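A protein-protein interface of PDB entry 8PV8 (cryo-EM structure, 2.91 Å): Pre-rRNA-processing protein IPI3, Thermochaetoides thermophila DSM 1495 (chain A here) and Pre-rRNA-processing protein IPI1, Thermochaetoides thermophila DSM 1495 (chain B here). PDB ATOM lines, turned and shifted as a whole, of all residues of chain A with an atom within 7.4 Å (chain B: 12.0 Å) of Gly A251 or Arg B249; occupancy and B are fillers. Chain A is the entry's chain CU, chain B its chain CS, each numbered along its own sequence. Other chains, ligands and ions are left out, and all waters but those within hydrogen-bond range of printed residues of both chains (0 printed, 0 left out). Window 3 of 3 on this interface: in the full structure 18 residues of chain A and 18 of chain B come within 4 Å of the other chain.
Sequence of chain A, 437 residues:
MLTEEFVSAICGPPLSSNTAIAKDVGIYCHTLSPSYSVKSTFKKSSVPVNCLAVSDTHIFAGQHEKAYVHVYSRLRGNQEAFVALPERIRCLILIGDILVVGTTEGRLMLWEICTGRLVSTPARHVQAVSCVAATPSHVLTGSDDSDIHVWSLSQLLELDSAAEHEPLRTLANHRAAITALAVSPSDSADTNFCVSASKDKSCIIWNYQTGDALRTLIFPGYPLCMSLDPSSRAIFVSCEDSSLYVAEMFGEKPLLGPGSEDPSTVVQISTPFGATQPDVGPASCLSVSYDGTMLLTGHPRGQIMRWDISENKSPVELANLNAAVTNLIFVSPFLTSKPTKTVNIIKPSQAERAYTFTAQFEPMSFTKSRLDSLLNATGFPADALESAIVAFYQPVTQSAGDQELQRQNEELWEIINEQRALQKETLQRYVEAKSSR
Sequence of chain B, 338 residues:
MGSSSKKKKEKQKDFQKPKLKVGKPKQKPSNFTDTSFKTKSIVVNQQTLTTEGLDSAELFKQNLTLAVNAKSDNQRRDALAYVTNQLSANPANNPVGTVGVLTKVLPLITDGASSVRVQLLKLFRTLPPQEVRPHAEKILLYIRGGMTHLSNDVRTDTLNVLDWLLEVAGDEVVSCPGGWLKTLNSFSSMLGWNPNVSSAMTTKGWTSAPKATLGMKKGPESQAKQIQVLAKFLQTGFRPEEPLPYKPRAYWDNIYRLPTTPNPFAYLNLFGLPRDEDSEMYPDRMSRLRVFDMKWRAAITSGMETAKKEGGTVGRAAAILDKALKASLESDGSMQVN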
ATOM      1  N   ARG A 233      29.380  17.362  -0.299  1.00  0.00           N
ATOM      2  CA  ARG A 233      29.374  16.161  -1.128  1.00  0.00           C
ATOM      3  C   ARG A 233      29.520  16.493  -2.609  1.00  0.00           C
ATOM      4  O   ARG A 233      29.957  15.650  -3.399  1.00  0.00           O
ATOM      5  CB  ARG A 233      28.087  15.364  -0.910  1.00  0.00           C
ATOM      6  CG  ARG A 233      27.785  14.968   0.522  1.00  0.00           C
ATOM      7  CD  ARG A 233      26.278  14.888   0.720  1.00  0.00           C
ATOM      8  NE  ARG A 233      25.894  14.126   1.901  1.00  0.00           N
ATOM      9  CZ  ARG A 233      24.680  14.142   2.432  1.00  0.00           C
ATOM     10  NH1 ARG A 233      23.712  14.884   1.921  1.00  0.00           N
ATOM     11  NH2 ARG A 233      24.430  13.395   3.504  1.00  0.00           N
ATOM     12  N   GLU A 248      30.149  15.143  -8.182  1.00  0.00           N
ATOM     13  CA  GLU A 248      30.032  14.458  -6.902  1.00  0.00           C
ATOM     14  C   GLU A 248      31.408  13.980  -6.458  1.00  0.00           C
ATOM     15  O   GLU A 248      32.133  13.357  -7.240  1.00  0.00           O
ATOM     16  CB  GLU A 248      29.053  13.289  -7.005  1.00  0.00           C
ATOM     17  CG  GLU A 248      28.276  13.026  -5.731  1.00  0.00           C
ATOM     18  CD  GLU A 248      27.092  12.111  -5.951  1.00  0.00           C
ATOM     19  OE1 GLU A 248      27.095  11.362  -6.951  1.00  0.00           O
ATOM     20  OE2 GLU A 248      26.160  12.136  -5.122  1.00  0.00           O
ATOM     21  N   MET A 249      31.765  14.289  -5.206  1.00  0.00           N
ATOM     22  CA  MET A 249      33.059  13.880  -4.668  1.00  0.00           C
ATOM     23  C   MET A 249      33.163  12.367  -4.539  1.00  0.00           C
ATOM     24  O   MET A 249      34.208  11.781  -4.843  1.00  0.00           O
ATOM     25  CB  MET A 249      33.283  14.525  -3.303  1.00  0.00           C
ATOM     26  CG  MET A 249      33.402  16.028  -3.305  1.00  0.00           C
ATOM     27  SD  MET A 249      34.838  16.596  -4.218  1.00  0.00           S
ATOM     28  CE  MET A 249      34.521  18.349  -4.199  1.00  0.00           C
ATOM     29  N   PHE A 250      32.093  11.716  -4.085  1.00  0.00           N
ATOM     30  CA  PHE A 250      32.150  10.330  -3.644  1.00  0.00           C
ATOM     31  C   PHE A 250      31.171   9.428  -4.388  1.00  0.00           C
ATOM     32  O   PHE A 250      30.477   8.625  -3.756  1.00  0.00           O
ATOM     33  CB  PHE A 250      31.896  10.262  -2.139  1.00  0.00           C
ATOM     34  CG  PHE A 250      32.662  11.286  -1.354  1.00  0.00           C
ATOM     35  CD1 PHE A 250      34.046  11.281  -1.347  1.00  0.00           C
ATOM     36  CD2 PHE A 250      31.998  12.273  -0.645  1.00  0.00           C
ATOM     37  CE1 PHE A 250      34.753  12.229  -0.631  1.00  0.00           C
ATOM     38  CE2 PHE A 250      32.699  13.225   0.069  1.00  0.00           C
ATOM     39  CZ  PHE A 250      34.078  13.202   0.076  1.00  0.00           C
ATOM     40  N   GLY A 251      31.100   9.540  -5.710  1.00  0.00           N
ATOM     41  CA  GLY A 251      30.191   8.714  -6.479  1.00  0.00           C
ATOM     42  C   GLY A 251      30.780   7.356  -6.809  1.00  0.00           C
ATOM     43  O   GLY A 251      31.679   6.846  -6.140  1.00  0.00           O
ATOM     44  N   GLU A 252      30.229   6.748  -7.865  1.00  0.00           N
ATOM     45  CA  GLU A 252      30.763   5.481  -8.357  1.00  0.00           C
ATOM     46  C   GLU A 252      32.180   5.653  -8.887  1.00  0.00           C
ATOM     47  O   GLU A 252      33.044   4.799  -8.665  1.00  0.00           O
ATOM     48  CB  GLU A 252      29.848   4.905  -9.437  1.00  0.00           C
ATOM     49  CG  GLU A 252      28.515   4.400  -8.912  1.00  0.00           C
ATOM     50  CD  GLU A 252      27.455   5.482  -8.873  1.00  0.00           C
ATOM     51  OE1 GLU A 252      27.732   6.605  -9.346  1.00  0.00           O
ATOM     52  OE2 GLU A 252      26.350   5.215  -8.359  1.00  0.00           O
ATOM     53  N   LYS A 253      32.431   6.751  -9.600  1.00  0.00           N
ATOM     54  CA  LYS A 253      33.785   7.165  -9.925  1.00  0.00           C
ATOM     55  C   LYS A 253      34.139   8.355  -9.052  1.00  0.00           C
ATOM     56  O   LYS A 253      33.875   9.500  -9.453  1.00  0.00           O
ATOM     57  CB  LYS A 253      33.902   7.535 -11.399  1.00  0.00           C
ATOM     58  CG  LYS A 253      33.626   6.385 -12.352  1.00  0.00           C
ATOM     59  CD  LYS A 253      34.659   5.283 -12.198  1.00  0.00           C
ATOM     60  CE  LYS A 253      36.011   5.722 -12.736  1.00  0.00           C
ATOM     61  NZ  LYS A 253      37.020   4.632 -12.664  1.00  0.00           N
ATOM     62  N   PRO A 254      34.718   8.147  -7.868  1.00  0.00           N
ATOM     63  CA  PRO A 254      34.874   9.256  -6.919  1.00  0.00           C
ATOM     64  C   PRO A 254      35.955  10.247  -7.317  1.00  0.00           C
ATOM     65  O   PRO A 254      37.055   9.860  -7.724  1.00  0.00           O
ATOM     66  CB  PRO A 254      35.225   8.543  -5.608  1.00  0.00           C
ATOM     67  CG  PRO A 254      35.886   7.287  -6.039  1.00  0.00           C
ATOM     68  CD  PRO A 254      35.229   6.876  -7.327  1.00  0.00           C
ATOM     69  N   LEU A 255      35.637  11.538  -7.208  1.00  0.00           N
ATOM     70  CA  LEU A 255      36.630  12.566  -7.496  1.00  0.00           C
ATOM     71  C   LEU A 255      37.649  12.664  -6.370  1.00  0.00           C
ATOM     72  O   LEU A 255      38.839  12.891  -6.616  1.00  0.00           O
ATOM     73  CB  LEU A 255      35.938  13.909  -7.722  1.00  0.00           C
ATOM     74  CG  LEU A 255      35.015  13.949  -8.941  1.00  0.00           C
ATOM     75  CD1 LEU A 255      34.287  15.281  -9.029  1.00  0.00           C
ATOM     76  CD2 LEU A 255      35.789  13.660 -10.215  1.00  0.00           C
ATOM     77  N   LEU A 256      37.201  12.492  -5.130  1.00  0.00           N
ATOM     78  CA  LEU A 256      38.071  12.479  -3.966  1.00  0.00           C
ATOM     79  C   LEU A 256      37.784  11.234  -3.143  1.00  0.00           C
ATOM     80  O   LEU A 256      36.776  10.551  -3.340  1.00  0.00           O
ATOM     81  CB  LEU A 256      37.884  13.733  -3.102  1.00  0.00           C
ATOM     82  CG  LEU A 256      38.322  15.065  -3.708  1.00  0.00           C
ATOM     83  CD1 LEU A 256      38.167  16.183  -2.692  1.00  0.00           C
ATOM     84  CD2 LEU A 256      39.756  14.982  -4.199  1.00  0.00           C
ATOM     85  N   LEU B 244      13.755  -4.743  -1.076  1.00  0.00           N
ATOM     86  CA  LEU B 244      14.850  -4.720  -2.036  1.00  0.00           C
ATOM     87  C   LEU B 244      16.019  -5.529  -1.492  1.00  0.00           C
ATOM     88  O   LEU B 244      16.280  -5.534  -0.288  1.00  0.00           O
ATOM     89  CB  LEU B 244      15.257  -3.270  -2.298  1.00  0.00           C
ATOM     90  CG  LEU B 244      16.330  -2.833  -3.301  1.00  0.00           C
ATOM     91  CD1 LEU B 244      15.955  -3.201  -4.731  1.00  0.00           C
ATOM     92  CD2 LEU B 244      16.591  -1.338  -3.185  1.00  0.00           C
ATOM     93  N   PRO B 245      16.751  -6.251  -2.359  1.00  0.00           N
ATOM     94  CA  PRO B 245      17.927  -6.997  -1.883  1.00  0.00           C
ATOM     95  C   PRO B 245      19.074  -6.113  -1.413  1.00  0.00           C
ATOM     96  O   PRO B 245      19.016  -4.884  -1.519  1.00  0.00           O
ATOM     97  CB  PRO B 245      18.331  -7.833  -3.105  1.00  0.00           C
ATOM     98  CG  PRO B 245      17.702  -7.146  -4.270  1.00  0.00           C
ATOM     99  CD  PRO B 245      16.408  -6.615  -3.743  1.00  0.00           C
ATOM    100  N   TYR B 246      20.127  -6.744  -0.896  1.00  0.00           N
ATOM    101  CA  TYR B 246      21.214  -6.047  -0.220  1.00  0.00           C
ATOM    102  C   TYR B 246      22.063  -5.277  -1.225  1.00  0.00           C
ATOM    103  O   TYR B 246      22.453  -5.819  -2.266  1.00  0.00           O
ATOM    104  CB  TYR B 246      22.082  -7.035   0.557  1.00  0.00           C
ATOM    105  CG  TYR B 246      23.325  -6.419   1.156  1.00  0.00           C
ATOM    106  CD1 TYR B 246      23.238  -5.375   2.065  1.00  0.00           C
ATOM    107  CD2 TYR B 246      24.588  -6.882   0.809  1.00  0.00           C
ATOM    108  CE1 TYR B 246      24.373  -4.808   2.615  1.00  0.00           C
ATOM    109  CE2 TYR B 246      25.729  -6.323   1.352  1.00  0.00           C
ATOM    110  CZ  TYR B 246      25.616  -5.287   2.255  1.00  0.00           C
ATOM    111  OH  TYR B 246      26.747  -4.725   2.797  1.00  0.00           O
ATOM    112  N   LYS B 247      22.347  -4.014  -0.907  1.00  0.00           N
ATOM    113  CA  LYS B 247      23.245  -3.191  -1.702  1.00  0.00           C
ATOM    114  C   LYS B 247      24.555  -3.023  -0.952  1.00  0.00           C
ATOM    115  O   LYS B 247      24.545  -2.506   0.176  1.00  0.00           O
ATOM    116  CB  LYS B 247      22.619  -1.833  -1.988  1.00  0.00           C
ATOM    117  CG  LYS B 247      23.391  -0.991  -2.989  1.00  0.00           C
ATOM    118  CD  LYS B 247      23.284  -1.562  -4.391  1.00  0.00           C
ATOM    119  CE  LYS B 247      23.834  -0.590  -5.422  1.00  0.00           C
ATOM    120  NZ  LYS B 247      25.297  -0.377  -5.255  1.00  0.00           N
ATOM    121  N   PRO B 248      25.687  -3.460  -1.514  1.00  0.00           N
ATOM    122  CA  PRO B 248      26.958  -3.416  -0.769  1.00  0.00           C
ATOM    123  C   PRO B 248      27.449  -2.017  -0.433  1.00  0.00           C
ATOM    124  O   PRO B 248      28.195  -1.868   0.542  1.00  0.00           O
ATOM    125  CB  PRO B 248      27.942  -4.124  -1.711  1.00  0.00           C
ATOM    126  CG  PRO B 248      27.084  -4.927  -2.629  1.00  0.00           C
ATOM    127  CD  PRO B 248      25.836  -4.128  -2.815  1.00  0.00           C
ATOM    128  N   ARG B 249      27.064  -0.994  -1.195  1.00  0.00           N
ATOM    129  CA  ARG B 249      27.562   0.359  -0.984  1.00  0.00           C
ATOM    130  C   ARG B 249      26.397   1.348  -0.895  1.00  0.00           C
ATOM    131  O   ARG B 249      26.375   2.397  -1.528  1.00  0.00           O
ATOM    132  CB  ARG B 249      28.552   0.756  -2.079  1.00  0.00           C
ATOM    133  CG  ARG B 249      28.065   0.563  -3.507  1.00  0.00           C
ATOM    134  CD  ARG B 249      29.032   1.214  -4.478  1.00  0.00           C
ATOM    135  NE  ARG B 249      29.079   2.658  -4.289  1.00  0.00           N
ATOM    136  CZ  ARG B 249      30.075   3.435  -4.691  1.00  0.00           C
ATOM    137  NH1 ARG B 249      31.128   2.938  -5.319  1.00  0.00           N
ATOM    138  NH2 ARG B 249      30.014   4.742  -4.456  1.00  0.00           N
ATOM    139  N   ALA B 250      25.395   1.015  -0.087  1.00  0.00           N
ATOM    140  CA  ALA B 250      24.296   1.931   0.169  1.00  0.00           C
ATOM    141  C   ALA B 250      24.411   2.675   1.490  1.00  0.00           C
ATOM    142  O   ALA B 250      24.044   3.856   1.540  1.00  0.00           O
ATOM    143  CB  ALA B 250      22.955   1.184   0.134  1.00  0.00           C
ATOM    144  N   TYR B 251      24.929   2.032   2.542  1.00  0.00           N
ATOM    145  CA  TYR B 251      25.015   2.654   3.860  1.00  0.00           C
ATOM    146  C   TYR B 251      25.940   3.866   3.849  1.00  0.00           C
ATOM    147  O   TYR B 251      25.615   4.910   4.426  1.00  0.00           O
ATOM    148  CB  TYR B 251      25.493   1.626   4.887  1.00  0.00           C
ATOM    149  CG  TYR B 251      25.874   2.210   6.230  1.00  0.00           C
ATOM    150  CD1 TYR B 251      24.902   2.604   7.138  1.00  0.00           C
ATOM    151  CD2 TYR B 251      27.207   2.353   6.595  1.00  0.00           C
ATOM    152  CE1 TYR B 251      25.247   3.132   8.365  1.00  0.00           C
ATOM    153  CE2 TYR B 251      27.558   2.882   7.821  1.00  0.00           C
ATOM    154  CZ  TYR B 251      26.573   3.269   8.701  1.00  0.00           C
ATOM    155  OH  TYR B 251      26.915   3.795   9.924  1.00  0.00           O
ATOM    156  N   TRP B 252      27.096   3.749   3.198  1.00  0.00           N
ATOM    157  CA  TRP B 252      28.029   4.866   3.156  1.00  0.00           C
ATOM    158  C   TRP B 252      27.665   5.893   2.094  1.00  0.00           C
ATOM    159  O   TRP B 252      27.969   7.078   2.269  1.00  0.00           O
ATOM    160  CB  TRP B 252      29.451   4.353   2.928  1.00  0.00           C
ATOM    161  CG  TRP B 252      30.113   3.881   4.186  1.00  0.00           C
ATOM    162  CD1 TRP B 252      30.509   2.608   4.473  1.00  0.00           C
ATOM    163  CD2 TRP B 252      30.452   4.674   5.332  1.00  0.00           C
ATOM    164  NE1 TRP B 252      31.073   2.558   5.723  1.00  0.00           N
ATOM    165  CE2 TRP B 252      31.052   3.814   6.271  1.00  0.00           C
ATOM    166  CE3 TRP B 252      30.310   6.028   5.652  1.00  0.00           C
ATOM    167  CZ2 TRP B 252      31.506   4.261   7.508  1.00  0.00           C
ATOM    168  CZ3 TRP B 252      30.761   6.469   6.880  1.00  0.00           C
ATOM    169  CH2 TRP B 252      31.352   5.589   7.793  1.00  0.00           C
ATOM    170  N   ASP B 253      27.023   5.471   1.006  1.00  0.00           N
ATOM    171  CA  ASP B 253      26.539   6.414   0.009  1.00  0.00           C
ATOM    172  C   ASP B 253      25.380   7.259   0.510  1.00  0.00           C
ATOM    173  O   ASP B 253      25.229   8.398   0.056  1.00  0.00           O
ATOM    174  CB  ASP B 253      26.130   5.679  -1.268  1.00  0.00           C
ATOM    175  CG  ASP B 253      27.321   5.225  -2.079  1.00  0.00           C
ATOM    176  OD1 ASP B 253      28.452   5.277  -1.551  1.00  0.00           O
ATOM    177  OD2 ASP B 253      27.130   4.817  -3.244  1.00  0.00           O
ATOM    178  N   ASN B 254      24.581   6.742   1.447  1.00  0.00           N
ATOM    179  CA  ASN B 254      23.563   7.540   2.119  1.00  0.00           C
ATOM    180  C   ASN B 254      24.146   8.717   2.893  1.00  0.00           C
ATOM    181  O   ASN B 254      23.435   9.700   3.124  1.00  0.00           O
ATOM    182  CB  ASN B 254      22.750   6.654   3.068  1.00  0.00           C
ATOM    183  CG  ASN B 254      21.496   7.337   3.574  1.00  0.00           C
ATOM    184  OD1 ASN B 254      20.818   8.043   2.829  1.00  0.00           O
ATOM    185  ND2 ASN B 254      21.186   7.134   4.848  1.00  0.00           N
ATOM    186  N   ILE B 255      25.417   8.647   3.281  1.00  0.00           N
ATOM    187  CA  ILE B 255      26.069   9.712   4.033  1.00  0.00           C
ATOM    188  C   ILE B 255      26.884  10.587   3.089  1.00  0.00           C
ATOM    189  O   ILE B 255      26.872  11.818   3.201  1.00  0.00           O
ATOM    190  CB  ILE B 255      26.951   9.125   5.151  1.00  0.00           C
ATOM    191  CG1 ILE B 255      26.142   8.150   6.007  1.00  0.00           C
ATOM    192  CG2 ILE B 255      27.535  10.225   6.013  1.00  0.00           C
ATOM    193  CD1 ILE B 255      26.945   7.482   7.096  1.00  0.00           C
ATOM    194  N   TYR B 256      27.585   9.964   2.144  1.00  0.00           N
ATOM    195  CA  TYR B 256      28.546  10.676   1.310  1.00  0.00           C
ATOM    196  C   TYR B 256      28.019  11.048  -0.071  1.00  0.00           C
ATOM    197  O   TYR B 256      28.800  11.526  -0.899  1.00  0.00           O
ATOM    198  CB  TYR B 256      29.823   9.846   1.161  1.00  0.00           C
ATOM    199  CG  TYR B 256      30.686   9.844   2.401  1.00  0.00           C
ATOM    200  CD1 TYR B 256      30.846  10.998   3.158  1.00  0.00           C
ATOM    201  CD2 TYR B 256      31.336   8.692   2.818  1.00  0.00           C
ATOM    202  CE1 TYR B 256      31.630  11.004   4.292  1.00  0.00           C
ATOM    203  CE2 TYR B 256      32.122   8.688   3.952  1.00  0.00           C
ATOM    204  CZ  TYR B 256      32.266   9.846   4.685  1.00  0.00           C
ATOM    205  OH  TYR B 256      33.049   9.849   5.815  1.00  0.00           O
ATOM    206  N   ARG B 257      26.733  10.848  -0.351  1.00  0.00           N
ATOM    207  CA  ARG B 257      26.160  11.238  -1.630  1.00  0.00           C
ATOM    208  C   ARG B 257      24.844  11.968  -1.411  1.00  0.00           C
ATOM    209  O   ARG B 257      24.214  11.847  -0.357  1.00  0.00           O
ATOM    210  CB  ARG B 257      25.943  10.030  -2.553  1.00  0.00           C
ATOM    211  CG  ARG B 257      27.230   9.378  -3.024  1.00  0.00           C
ATOM    212  CD  ARG B 257      26.961   8.177  -3.908  1.00  0.00           C
ATOM    213  NE  ARG B 257      26.355   8.543  -5.181  1.00  0.00           N
ATOM    214  CZ  ARG B 257      26.040   7.676  -6.132  1.00  0.00           C
ATOM    215  NH1 ARG B 257      26.262   6.381  -5.987  1.00  0.00           N
ATOM    216  NH2 ARG B 257      25.489   8.119  -7.259  1.00  0.00           N
ATOM    217  N   LEU B 258      24.447  12.738  -2.420  1.00  0.00           N
ATOM    218  CA  LEU B 258      23.224  13.518  -2.347  1.00  0.00           C
ATOM    219  C   LEU B 258      22.002  12.600  -2.332  1.00  0.00           C
ATOM    220  O   LEU B 258      22.040  11.497  -2.887  1.00  0.00           O
ATOM    221  CB  LEU B 258      23.140  14.478  -3.531  1.00  0.00           C
ATOM    222  CG  LEU B 258      24.185  15.592  -3.571  1.00  0.00           C
ATOM    223  CD1 LEU B 258      24.059  16.379  -4.860  1.00  0.00           C
ATOM    224  CD2 LEU B 258      24.042  16.502  -2.367  1.00  0.00           C
ATOM    225  N   PRO B 259      20.915  13.022  -1.686  1.00  0.00           N
ATOM    226  CA  PRO B 259      19.705  12.189  -1.659  1.00  0.00           C
ATOM    227  C   PRO B 259      19.063  12.088  -3.037  1.00  0.00           C
ATOM    228  O   PRO B 259      18.809  13.097  -3.699  1.00  0.00           O
ATOM    229  CB  PRO B 259      18.795  12.922  -0.666  1.00  0.00           C
ATOM    230  CG  PRO B 259      19.725  13.751   0.160  1.00  0.00           C
ATOM    231  CD  PRO B 259      20.795  14.181  -0.787  1.00  0.00           C
ATOM    232  N   THR B 260      18.805  10.854  -3.464  1.00  0.00           N
ATOM    233  CA  THR B 260      18.177  10.584  -4.749  1.00  0.00           C
ATOM    234  C   THR B 260      16.665  10.434  -4.651  1.00  0.00           C
ATOM    235  O   THR B 260      16.005  10.268  -5.681  1.00  0.00           O
ATOM    236  CB  THR B 260      18.776   9.321  -5.375  1.00  0.00           C
ATOM    237  OG1 THR B 260      18.452   8.185  -4.564  1.00  0.00           O
ATOM    238  CG2 THR B 260      20.287   9.446  -5.483  1.00  0.00           C
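N of Met A249 lies within hydrogen-bond range of O of Arg A233, at 2.9 Å. OD2 of Asp B253 is in salt-bridge range of NE of Arg B249 (3.1 Å). The side-chain carboxylate (OD2) of Asp B253 is in salt-bridge range of the guanidinium group (NH1) of Arg B257 (3.3 Å).
The backbone carbonyl oxygen (O) of Ile B255 is in hydrogen-bond range of the guanidinium group (NE) of Arg A233 (2.8 Å). The side-chain carboxylate (OE1) of Glu A248 is in salt-bridge range of the guanidinium group (NE) of Arg B257, 3.4 Å away. The side-chain carboxylate (OE2) of Glu A248 lies within hydrogen-bond range of the backbone NH (N) of Leu B258, 3.3 Å away. The guanidinium group (NH2) of Arg B249 sits at hydrogen-bond distance from the backbone carbonyl oxygen (O) of Gly A251 (3.2 Å). The side-chain carboxylate (OE2) of Glu A252 is in salt-bridge range of the guanidinium group (NH1) of Arg B257, 2.6 Å away.
Among the printed residues, pairs that only touch across the chains: Arg A233 with Asn B254, Arg A233 with Tyr B256, Arg A233 with Arg B257, Phe A250 with Arg B249, Phe A250 with Tyr B256, Phe A250 with Arg B257 and Glu A252 with Arg B249.
Of the 17 printed residues of chain B, 6 touch a printed residue of chain A. Hydrophobic or aromatic side chains of chain B that line the printed part of chain A: Tyr B256. Of the 10 printed residues of chain A, 5 touch a printed residue of chain B. Hydrophobic or aromatic side chains of chain A within 4 Å of the printed part of chain B: Phe A250. Among the printed residues, 12 pairs touch across the chains. Among the printed residues, Asp or Glu carboxylates within 4 Å of a Lys or Arg side-chain nitrogen of the other chain: Glu A248 with Arg B257 (3.4 Å) and Glu A252 with Arg B257 (2.6 Å).
Printed residues of chain B within 4 Å of Glu A248: Arg B257 and Leu B258. Of chain B, only Arg B249 (3.97 Å), Tyr B256 (3.3 Å) and Arg B257 (3.4 Å) come within 4 Å of Phe A250. Glu A252 touches just these residues of chain B: Arg B249 and Arg B257. No residue of chain B comes within 4 Å of Pro A254. Leu A255 touches none of the printed residues of chain B. Arg B249 touches three residues of chain A. Of the printed residues of chain A, Asn B254 touches Arg A233. Printed residues of chain A within 4 Å of Arg B257: Arg A233, Glu A248, Phe A250 and Glu A252. Of the printed residues of chain A, Leu B258 touches Glu A248. The nearest printed residue of chain A that does not touch Arg B257 is Gly A251 (4.1 Å).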
